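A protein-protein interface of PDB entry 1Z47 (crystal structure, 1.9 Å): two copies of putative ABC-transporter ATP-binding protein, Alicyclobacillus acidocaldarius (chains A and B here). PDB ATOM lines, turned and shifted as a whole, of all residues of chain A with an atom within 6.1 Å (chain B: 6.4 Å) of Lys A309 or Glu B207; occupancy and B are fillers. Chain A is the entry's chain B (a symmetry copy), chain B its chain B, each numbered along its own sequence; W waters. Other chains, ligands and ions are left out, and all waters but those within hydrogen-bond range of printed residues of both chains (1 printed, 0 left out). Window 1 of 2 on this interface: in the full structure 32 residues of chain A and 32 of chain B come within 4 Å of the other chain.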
ATOM      1  N   ARG A 182       5.997  19.584 -45.084  1.00  0.00           N
ATOM      2  CA  ARG A 182       4.692  19.031 -44.763  1.00  0.00           C
ATOM      3  C   ARG A 182       3.788  18.950 -45.987  1.00  0.00           C
ATOM      4  O   ARG A 182       3.034  17.977 -46.144  1.00  0.00           O
ATOM      5  CB  ARG A 182       4.012  19.846 -43.651  1.00  0.00           C
ATOM      6  CG  ARG A 182       4.693  19.701 -42.289  1.00  0.00           C
ATOM      7  CD  ARG A 182       3.839  20.261 -41.165  1.00  0.00           C
ATOM      8  NE  ARG A 182       4.673  20.762 -40.075  1.00  0.00           N
ATOM      9  CZ  ARG A 182       4.206  21.242 -38.922  1.00  0.00           C
ATOM     10  NH1 ARG A 182       2.894  21.289 -38.696  1.00  0.00           N
ATOM     11  NH2 ARG A 182       5.055  21.680 -37.993  1.00  0.00           N
ATOM     12  N   GLU A 207       6.553  11.485 -35.930  1.00  0.00           N
ATOM     13  CA  GLU A 207       5.301  12.107 -36.354  1.00  0.00           C
ATOM     14  C   GLU A 207       5.088  11.889 -37.844  1.00  0.00           C
ATOM     15  O   GLU A 207       3.983  11.576 -38.278  1.00  0.00           O
ATOM     16  CB  GLU A 207       5.309  13.610 -36.058  1.00  0.00           C
ATOM     17  CG  GLU A 207       3.917  14.210 -35.917  1.00  0.00           C
ATOM     18  CD  GLU A 207       3.689  15.367 -36.861  1.00  0.00           C
ATOM     19  OE1 GLU A 207       3.424  15.112 -38.054  1.00  0.00           O
ATOM     20  OE2 GLU A 207       3.782  16.535 -36.413  1.00  0.00           O
ATOM     21  N   GLU A 248       4.864  11.052 -27.673  1.00  0.00           N
ATOM     22  CA  GLU A 248       5.621  11.751 -26.652  1.00  0.00           C
ATOM     23  C   GLU A 248       5.461  11.000 -25.344  1.00  0.00           C
ATOM     24  O   GLU A 248       4.452  10.316 -25.139  1.00  0.00           O
ATOM     25  CB  GLU A 248       5.103  13.179 -26.545  1.00  0.00           C
ATOM     26  CG  GLU A 248       5.511  13.998 -27.780  1.00  0.00           C
ATOM     27  CD  GLU A 248       4.831  15.347 -27.873  1.00  0.00           C
ATOM     28  OE1 GLU A 248       3.762  15.423 -28.520  1.00  0.00           O
ATOM     29  OE2 GLU A 248       5.366  16.325 -27.300  1.00  0.00           O
ATOM     30  N   ALA A 307       3.144  26.609 -22.214  1.00  0.00           N
ATOM     31  CA  ALA A 307       3.329  27.131 -23.567  1.00  0.00           C
ATOM     32  C   ALA A 307       2.096  26.754 -24.384  1.00  0.00           C
ATOM     33  O   ALA A 307       1.721  25.592 -24.470  1.00  0.00           O
ATOM     34  CB  ALA A 307       4.604  26.546 -24.219  1.00  0.00           C
ATOM     35  N   PHE A 308       1.461  27.763 -24.967  1.00  0.00           N
ATOM     36  CA  PHE A 308       0.277  27.542 -25.770  1.00  0.00           C
ATOM     37  C   PHE A 308       0.690  26.948 -27.111  1.00  0.00           C
ATOM     38  O   PHE A 308       1.429  27.578 -27.865  1.00  0.00           O
ATOM     39  CB  PHE A 308      -0.446  28.872 -26.005  1.00  0.00           C
ATOM     40  CG  PHE A 308      -1.684  28.735 -26.831  1.00  0.00           C
ATOM     41  CD1 PHE A 308      -2.773  28.018 -26.353  1.00  0.00           C
ATOM     42  CD2 PHE A 308      -1.741  29.260 -28.120  1.00  0.00           C
ATOM     43  CE1 PHE A 308      -3.903  27.815 -27.146  1.00  0.00           C
ATOM     44  CE2 PHE A 308      -2.871  29.061 -28.921  1.00  0.00           C
ATOM     45  CZ  PHE A 308      -3.950  28.340 -28.435  1.00  0.00           C
ATOM     46  N   LYS A 309       0.191  25.766 -27.447  1.00  0.00           N
ATOM     47  CA  LYS A 309       0.598  25.182 -28.723  1.00  0.00           C
ATOM     48  C   LYS A 309      -0.532  25.020 -29.736  1.00  0.00           C
ATOM     49  O   LYS A 309      -0.410  24.285 -30.711  1.00  0.00           O
ATOM     50  CB  LYS A 309       1.325  23.855 -28.467  1.00  0.00           C
ATOM     51  CG  LYS A 309       2.594  24.058 -27.601  1.00  0.00           C
ATOM     52  CD  LYS A 309       3.495  22.854 -27.625  1.00  0.00           C
ATOM     53  CE  LYS A 309       4.143  22.683 -28.985  1.00  0.00           C
ATOM     54  NZ  LYS A 309       4.912  21.417 -29.035  1.00  0.00           N
ATOM     55  N   GLY A 310      -1.632  25.727 -29.504  1.00  0.00           N
ATOM     56  CA  GLY A 310      -2.762  25.669 -30.418  1.00  0.00           C
ATOM     57  C   GLY A 310      -3.868  24.737 -29.993  1.00  0.00           C
ATOM     58  O   GLY A 310      -4.833  25.156 -29.361  1.00  0.00           O
ATOM     59  N   SER A 311      -3.731  23.465 -30.349  1.00  0.00           N
ATOM     60  CA  SER A 311      -4.712  22.446 -30.000  1.00  0.00           C
ATOM     61  C   SER A 311      -4.614  22.048 -28.534  1.00  0.00           C
ATOM     62  O   SER A 311      -5.487  21.353 -28.018  1.00  0.00           O
ATOM     63  CB  SER A 311      -4.495  21.195 -30.854  1.00  0.00           C
ATOM     64  OG  SER A 311      -5.135  20.081 -30.264  1.00  0.00           O
ATOM     65  N   TYR A 312      -3.540  22.475 -27.876  1.00  0.00           N
ATOM     66  CA  TYR A 312      -3.336  22.138 -26.469  1.00  0.00           C
ATOM     67  C   TYR A 312      -2.268  23.033 -25.881  1.00  0.00           C
ATOM     68  O   TYR A 312      -1.491  23.655 -26.611  1.00  0.00           O
ATOM     69  CB  TYR A 312      -2.905  20.667 -26.344  1.00  0.00           C
ATOM     70  CG  TYR A 312      -1.492  20.407 -26.826  1.00  0.00           C
ATOM     71  CD1 TYR A 312      -0.406  20.577 -25.967  1.00  0.00           C
ATOM     72  CD2 TYR A 312      -1.230  20.070 -28.164  1.00  0.00           C
ATOM     73  CE1 TYR A 312       0.910  20.427 -26.415  1.00  0.00           C
ATOM     74  CE2 TYR A 312       0.099  19.920 -28.627  1.00  0.00           C
ATOM     75  CZ  TYR A 312       1.159  20.104 -27.738  1.00  0.00           C
ATOM     76  OH  TYR A 312       2.466  19.987 -28.166  1.00  0.00           O
ATOM     77  N   SER A 313      -2.246  23.108 -24.555  1.00  0.00           N
ATOM     78  CA  SER A 313      -1.263  23.889 -23.845  1.00  0.00           C
ATOM     79  C   SER A 313      -0.277  22.911 -23.186  1.00  0.00           C
ATOM     80  O   SER A 313      -0.680  21.922 -22.558  1.00  0.00           O
ATOM     81  CB  SER A 313      -1.947  24.746 -22.775  1.00  0.00           C
ATOM     82  OG  SER A 313      -1.015  25.574 -22.083  1.00  0.00           O
ATOM     83  N   ALA A 314       1.010  23.178 -23.344  1.00  0.00           N
ATOM     84  CA  ALA A 314       2.017  22.312 -22.758  1.00  0.00           C
ATOM     85  C   ALA A 314       2.363  22.862 -21.387  1.00  0.00           C
ATOM     86  O   ALA A 314       2.626  24.056 -21.231  1.00  0.00           O
ATOM     87  CB  ALA A 314       3.270  22.262 -23.641  1.00  0.00           C
ATOM     88  N   TRP A 316       4.890  22.191 -18.046  1.00  0.00           N
ATOM     89  CA  TRP A 316       5.987  21.490 -17.390  1.00  0.00           C
ATOM     90  C   TRP A 316       5.894  21.720 -15.876  1.00  0.00           C
ATOM     91  O   TRP A 316       5.763  22.859 -15.417  1.00  0.00           O
ATOM     92  CB  TRP A 316       7.337  21.991 -17.913  1.00  0.00           C
ATOM     93  CG  TRP A 316       7.618  21.506 -19.323  1.00  0.00           C
ATOM     94  CD1 TRP A 316       8.196  20.318 -19.689  1.00  0.00           C
ATOM     95  CD2 TRP A 316       7.241  22.161 -20.541  1.00  0.00           C
ATOM     96  NE1 TRP A 316       8.196  20.190 -21.063  1.00  0.00           N
ATOM     97  CE2 TRP A 316       7.614  21.308 -21.610  1.00  0.00           C
ATOM     98  CE3 TRP A 316       6.613  23.381 -20.834  1.00  0.00           C
ATOM     99  CZ2 TRP A 316       7.384  21.642 -22.954  1.00  0.00           C
ATOM    100  CZ3 TRP A 316       6.382  23.714 -22.174  1.00  0.00           C
ATOM    101  CH2 TRP A 316       6.768  22.840 -23.214  1.00  0.00           C
ATOM    102  N   GLU A 326       6.164  16.601 -18.368  1.00  0.00           N
ATOM    103  CA  GLU A 326       5.510  17.394 -19.396  1.00  0.00           C
ATOM    104  C   GLU A 326       4.080  16.884 -19.469  1.00  0.00           C
ATOM    105  O   GLU A 326       3.834  15.691 -19.601  1.00  0.00           O
ATOM    106  CB  GLU A 326       6.170  17.244 -20.780  1.00  0.00           C
ATOM    107  CG  GLU A 326       5.461  18.122 -21.836  1.00  0.00           C
ATOM    108  CD  GLU A 326       6.124  18.111 -23.210  1.00  0.00           C
ATOM    109  OE1 GLU A 326       7.282  17.659 -23.321  1.00  0.00           O
ATOM    110  OE2 GLU A 326       5.482  18.577 -24.176  1.00  0.00           O
ATOM    111  N   HIS A 328       0.076  17.721 -21.158  1.00  0.00           N
ATOM    112  CA  HIS A 328      -0.665  18.435 -22.194  1.00  0.00           C
ATOM    113  C   HIS A 328      -2.104  18.648 -21.729  1.00  0.00           C
ATOM    114  O   HIS A 328      -2.833  17.687 -21.523  1.00  0.00           O
ATOM    115  CB  HIS A 328      -0.637  17.643 -23.512  1.00  0.00           C
ATOM    116  CG  HIS A 328       0.709  17.629 -24.177  1.00  0.00           C
ATOM    117  ND1 HIS A 328       0.950  16.967 -25.361  1.00  0.00           N
ATOM    118  CD2 HIS A 328       1.878  18.228 -23.834  1.00  0.00           C
ATOM    119  CE1 HIS A 328       2.211  17.154 -25.716  1.00  0.00           C
ATOM    120  NE2 HIS A 328       2.796  17.916 -24.808  1.00  0.00           N
ATOM    121  N   LEU B  47      10.824  33.774 -36.485  1.00  0.00           N
ATOM    122  CA  LEU B  47      10.159  32.771 -37.320  1.00  0.00           C
ATOM    123  C   LEU B  47       9.802  33.250 -38.729  1.00  0.00           C
ATOM    124  O   LEU B  47       9.071  34.234 -38.892  1.00  0.00           O
ATOM    125  CB  LEU B  47       8.896  32.304 -36.592  1.00  0.00           C
ATOM    126  CG  LEU B  47       7.894  31.422 -37.338  1.00  0.00           C
ATOM    127  CD1 LEU B  47       8.557  30.104 -37.772  1.00  0.00           C
ATOM    128  CD2 LEU B  47       6.705  31.137 -36.426  1.00  0.00           C
ATOM    129  N   ARG B 182      14.319  17.757 -29.864  1.00  0.00           N
ATOM    130  CA  ARG B 182      13.275  18.124 -28.922  1.00  0.00           C
ATOM    131  C   ARG B 182      13.788  18.175 -27.488  1.00  0.00           C
ATOM    132  O   ARG B 182      13.389  19.056 -26.712  1.00  0.00           O
ATOM    133  CB  ARG B 182      12.081  17.161 -29.028  1.00  0.00           C
ATOM    134  CG  ARG B 182      11.303  17.299 -30.338  1.00  0.00           C
ATOM    135  CD  ARG B 182       9.974  16.566 -30.289  1.00  0.00           C
ATOM    136  NE  ARG B 182       9.585  16.100 -31.618  1.00  0.00           N
ATOM    137  CZ  ARG B 182       8.433  15.492 -31.902  1.00  0.00           C
ATOM    138  NH1 ARG B 182       7.536  15.271 -30.941  1.00  0.00           N
ATOM    139  NH2 ARG B 182       8.178  15.101 -33.150  1.00  0.00           N
ATOM    140  N   ARG B 185      15.829  21.512 -27.197  1.00  0.00           N
ATOM    141  CA  ARG B 185      15.106  22.769 -27.032  1.00  0.00           C
ATOM    142  C   ARG B 185      14.565  22.894 -25.614  1.00  0.00           C
ATOM    143  O   ARG B 185      14.508  23.988 -25.083  1.00  0.00           O
ATOM    144  CB  ARG B 185      13.961  22.891 -28.036  1.00  0.00           C
ATOM    145  CG  ARG B 185      12.867  21.889 -27.841  1.00  0.00           C
ATOM    146  CD  ARG B 185      11.655  22.243 -28.706  1.00  0.00           C
ATOM    147  NE  ARG B 185      10.847  21.072 -29.033  1.00  0.00           N
ATOM    148  CZ  ARG B 185      10.435  20.155 -28.156  1.00  0.00           C
ATOM    149  NH1 ARG B 185      10.747  20.254 -26.869  1.00  0.00           N
ATOM    150  NH2 ARG B 185       9.707  19.124 -28.575  1.00  0.00           N
ATOM    151  N   ASP B 205      10.332  26.588 -38.198  1.00  0.00           N
ATOM    152  CA  ASP B 205       9.375  25.631 -37.617  1.00  0.00           C
ATOM    153  C   ASP B 205       8.435  26.333 -36.622  1.00  0.00           C
ATOM    154  O   ASP B 205       8.807  26.600 -35.482  1.00  0.00           O
ATOM    155  CB  ASP B 205      10.138  24.521 -36.879  1.00  0.00           C
ATOM    156  CG  ASP B 205       9.221  23.413 -36.373  1.00  0.00           C
ATOM    157  OD1 ASP B 205       7.989  23.640 -36.262  1.00  0.00           O
ATOM    158  OD2 ASP B 205       9.742  22.308 -36.087  1.00  0.00           O
ATOM    159  N   GLN B 206       7.204  26.602 -37.038  1.00  0.00           N
ATOM    160  CA  GLN B 206       6.302  27.313 -36.153  1.00  0.00           C
ATOM    161  C   GLN B 206       6.038  26.576 -34.842  1.00  0.00           C
ATOM    162  O   GLN B 206       5.863  27.209 -33.805  1.00  0.00           O
ATOM    163  CB  GLN B 206       4.992  27.639 -36.887  1.00  0.00           C
ATOM    164  CG  GLN B 206       4.204  26.441 -37.436  1.00  0.00           C
ATOM    165  CD  GLN B 206       3.398  25.721 -36.369  1.00  0.00           C
ATOM    166  OE1 GLN B 206       2.815  26.349 -35.476  1.00  0.00           O
ATOM    167  NE2 GLN B 206       3.331  24.404 -36.474  1.00  0.00           N
ATOM    168  N   GLU B 207       6.036  25.246 -34.867  1.00  0.00           N
ATOM    169  CA  GLU B 207       5.783  24.505 -33.633  1.00  0.00           C
ATOM    170  C   GLU B 207       6.876  24.792 -32.616  1.00  0.00           C
ATOM    171  O   GLU B 207       6.597  24.995 -31.438  1.00  0.00           O
ATOM    172  CB  GLU B 207       5.724  22.998 -33.902  1.00  0.00           C
ATOM    173  CG  GLU B 207       4.923  22.224 -32.865  1.00  0.00           C
ATOM    174  CD  GLU B 207       5.723  21.112 -32.228  1.00  0.00           C
ATOM    175  OE1 GLU B 207       6.538  21.411 -31.331  1.00  0.00           O
ATOM    176  OE2 GLU B 207       5.545  19.937 -32.631  1.00  0.00           O
ATOM    177  N   GLU B 208       8.126  24.814 -33.077  1.00  0.00           N
ATOM    178  CA  GLU B 208       9.253  25.099 -32.191  1.00  0.00           C
ATOM    179  C   GLU B 208       9.107  26.498 -31.583  1.00  0.00           C
ATOM    180  O   GLU B 208       9.385  26.708 -30.398  1.00  0.00           O
ATOM    181  CB  GLU B 208      10.574  25.023 -32.954  1.00  0.00           C
ATOM    182  CG  GLU B 208      11.769  25.437 -32.120  1.00  0.00           C
ATOM    183  CD  GLU B 208      13.093  25.404 -32.880  1.00  0.00           C
ATOM    184  OE1 GLU B 208      13.107  25.658 -34.106  1.00  0.00           O
ATOM    185  OE2 GLU B 208      14.134  25.140 -32.233  1.00  0.00           O
ATOM    186  N   ALA B 209       8.674  27.451 -32.401  1.00  0.00           N
ATOM    187  CA  ALA B 209       8.503  28.818 -31.917  1.00  0.00           C
ATOM    188  C   ALA B 209       7.434  28.891 -30.813  1.00  0.00           C
ATOM    189  O   ALA B 209       7.647  29.510 -29.780  1.00  0.00           O
ATOM    190  CB  ALA B 209       8.148  29.747 -33.083  1.00  0.00           C
ATOM    191  N   LEU B 210       6.290  28.261 -31.024  1.00  0.00           N
ATOM    192  CA  LEU B 210       5.229  28.291 -30.013  1.00  0.00           C
ATOM    193  C   LEU B 210       5.673  27.619 -28.725  1.00  0.00           C
ATOM    194  O   LEU B 210       5.300  28.031 -27.620  1.00  0.00           O
ATOM    195  CB  LEU B 210       3.969  27.561 -30.498  1.00  0.00           C
ATOM    196  CG  LEU B 210       3.205  28.094 -31.720  1.00  0.00           C
ATOM    197  CD1 LEU B 210       2.116  27.072 -32.097  1.00  0.00           C
ATOM    198  CD2 LEU B 210       2.590  29.463 -31.431  1.00  0.00           C
ATOM    199  N   GLU B 211       6.459  26.563 -28.878  1.00  0.00           N
ATOM    200  CA  GLU B 211       6.917  25.799 -27.737  1.00  0.00           C
ATOM    201  C   GLU B 211       7.880  26.481 -26.781  1.00  0.00           C
ATOM    202  O   GLU B 211       7.738  26.351 -25.558  1.00  0.00           O
ATOM    203  CB  GLU B 211       7.571  24.516 -28.209  1.00  0.00           C
ATOM    204  CG  GLU B 211       8.308  23.820 -27.091  1.00  0.00           C
ATOM    205  CD  GLU B 211       7.699  22.497 -26.721  1.00  0.00           C
ATOM    206  OE1 GLU B 211       6.465  22.322 -26.863  1.00  0.00           O
ATOM    207  OE2 GLU B 211       8.468  21.633 -26.268  1.00  0.00           O
ATOM    208  N   VAL B 212       8.870  27.190 -27.314  1.00  0.00           N
ATOM    209  CA  VAL B 212       9.845  27.796 -26.426  1.00  0.00           C
ATOM    210  C   VAL B 212       9.902  29.309 -26.335  1.00  0.00           C
ATOM    211  O   VAL B 212      10.443  29.824 -25.369  1.00  0.00           O
ATOM    212  CB  VAL B 212      11.282  27.281 -26.740  1.00  0.00           C
ATOM    213  CG1 VAL B 212      11.322  25.749 -26.687  1.00  0.00           C
ATOM    214  CG2 VAL B 212      11.722  27.764 -28.082  1.00  0.00           C
ATOM    215  N   PRO B 230       2.755  33.402 -28.337  1.00  0.00           N
ATOM    216  CA  PRO B 230       2.299  32.222 -29.074  1.00  0.00           C
ATOM    217  C   PRO B 230       0.784  32.248 -29.246  1.00  0.00           C
ATOM    218  O   PRO B 230       0.258  31.959 -30.324  1.00  0.00           O
ATOM    219  CB  PRO B 230       2.751  31.067 -28.176  1.00  0.00           C
ATOM    220  CG  PRO B 230       4.061  31.557 -27.674  1.00  0.00           C
ATOM    221  CD  PRO B 230       3.731  33.014 -27.300  1.00  0.00           C
ATOM    222  N   TYR B 234      -1.286  32.826 -32.819  1.00  0.00           N
ATOM    223  CA  TYR B 234      -2.124  31.689 -33.193  1.00  0.00           C
ATOM    224  C   TYR B 234      -3.620  32.011 -33.219  1.00  0.00           C
ATOM    225  O   TYR B 234      -4.333  31.627 -34.155  1.00  0.00           O
ATOM    226  CB  TYR B 234      -1.907  30.513 -32.224  1.00  0.00           C
ATOM    227  CG  TYR B 234      -2.628  29.222 -32.603  1.00  0.00           C
ATOM    228  CD1 TYR B 234      -1.978  28.204 -33.313  1.00  0.00           C
ATOM    229  CD2 TYR B 234      -3.950  29.006 -32.225  1.00  0.00           C
ATOM    230  CE1 TYR B 234      -2.638  27.004 -33.630  1.00  0.00           C
ATOM    231  CE2 TYR B 234      -4.607  27.819 -32.532  1.00  0.00           C
ATOM    232  CZ  TYR B 234      -3.953  26.823 -33.231  1.00  0.00           C
ATOM    233  OH  TYR B 234      -4.618  25.650 -33.494  1.00  0.00           O
ATOM    234  N   GLY B 247       0.516  27.400 -36.751  1.00  0.00           N
ATOM    235  CA  GLY B 247      -0.504  26.378 -36.580  1.00  0.00           C
ATOM    236  C   GLY B 247      -0.761  25.753 -37.937  1.00  0.00           C
ATOM    237  O   GLY B 247      -0.048  26.025 -38.901  1.00  0.00           O
HETATM  238  O   HOH W   1       2.048  21.337 -35.480  1.00  0.00           O
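The side-chain amino group of Lys A309 is in salt-bridge range of the side-chain carboxylate of Glu B207 (2.8 Å).
The side-chain carboxylate of Glu B211 lies within salt-bridge range of the side-chain amino group of Lys A309 (2.8 Å).
The side-chain carboxylate of Asp B205 lies within salt-bridge range of the guanidinium group of Arg A182, at 3.9 Å.
O of Arg B182 sits at hydrogen-bond distance from NH1 of Arg B185 (2.9 Å).
The guanidinium group (NH1) of Arg B185 lies within salt-bridge range of the side-chain carboxylate (OE2) of Glu B211 (2.7 Å).
OE1 of Gln B206 lies within hydrogen-bond range of N of Gly B247.
The backbone carbonyl oxygen of Ala A307 is in hydrogen-bond range of the backbone NH of Ala A314, at 2.8 Å.
OD1 of Asp B205 sits at hydrogen-bond distance from N of Glu B208, 3.4 Å away.
The side-chain amino group of Lys A309 sits at hydrogen-bond distance from the side-chain hydroxyl of Tyr A312 (3.0 Å).
Water W1 lies within hydrogen-bond range of NH1 of Arg A182 and NE2 of Gln B206.
Printed residues of chain B within 4 Å of Lys A309: Glu B207 (2.8 Å) and Glu B211 (2.8 Å).
Glu B207 touches just one residue of chain A: Lys A309 (2.8 Å).
Of the printed residues of chain A, Pro B230 touches Phe A308.
Printed residues of chain B within 4 Å of Glu A248: Arg B182.
Of the printed residues of chain B, Ala A307 touches Leu B210 and Glu B211.
Of the printed residues of chain A, Tyr B234 touches Phe A308 (3.5 Å), Gly A310 (3.3 Å) and Ser A311 (3.9 Å).
Glu B208 touches none of the printed residues of chain A.
The nearest printed residue of chain B that does not touch Lys A309 is Leu B210 (4.01 Å).
The nearest printed residue of chain A that does not touch Arg B182 is Glu A207 (4.3 Å).
Of the 14 printed residues of chain B, 8 touch a printed residue of chain A.
Printed residues of chain B that touch a printed residue of chain A: Arg B182, Asp B205, Gln B206, Glu B207, Leu B210, Glu B211, Pro B230 and Tyr B234.
Hydrophobic or aromatic side chains of chain B within 4 Å of the printed part of chain A: Leu B210, Pro B230 and Tyr B234.
Of the 14 printed residues of chain A, 8 touch a printed residue of chain B.
Printed residues of chain A that touch a printed residue of chain B: Arg A182, Glu A248, Ala A307, Phe A308, Lys A309, Gly A310, Ser A311 and Trp A316.
Hydrophobic or aromatic side chains of chain A that line the printed part of chain B: Ala A307, Phe A308 and Trp A316.
Among the printed residues, Asp or Glu carboxylates within 4 Å of a Lys or Arg side-chain nitrogen of the other chain: Arg A182 with Asp B205, Lys A309 with Glu B207 and Lys A309 with Glu B211.
Arg A182 touches Gln B206.
Glu A248 touches Arg B182.
O of Leu B210 touches CB of Ala A307, 3.8 Å away.
CB of Ala A307 touches O of Glu B211, at 3.4 Å.
Phe A308 touches Leu B210.
Phe A308 touches Pro B230 (O to CB, 3.7 Å).
Phe A308 touches Tyr B234.
Tyr B234 touches Gly A310.
Tyr B234 touches Ser A311.
OE2 of Glu B211 touches CZ2 of Trp A316, at 3.5 Å.
2 positions are printed for both chains.
Of the 13 pairs that touch across the chains among the printed residues, none has its exchanged pair printed and touching as well.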
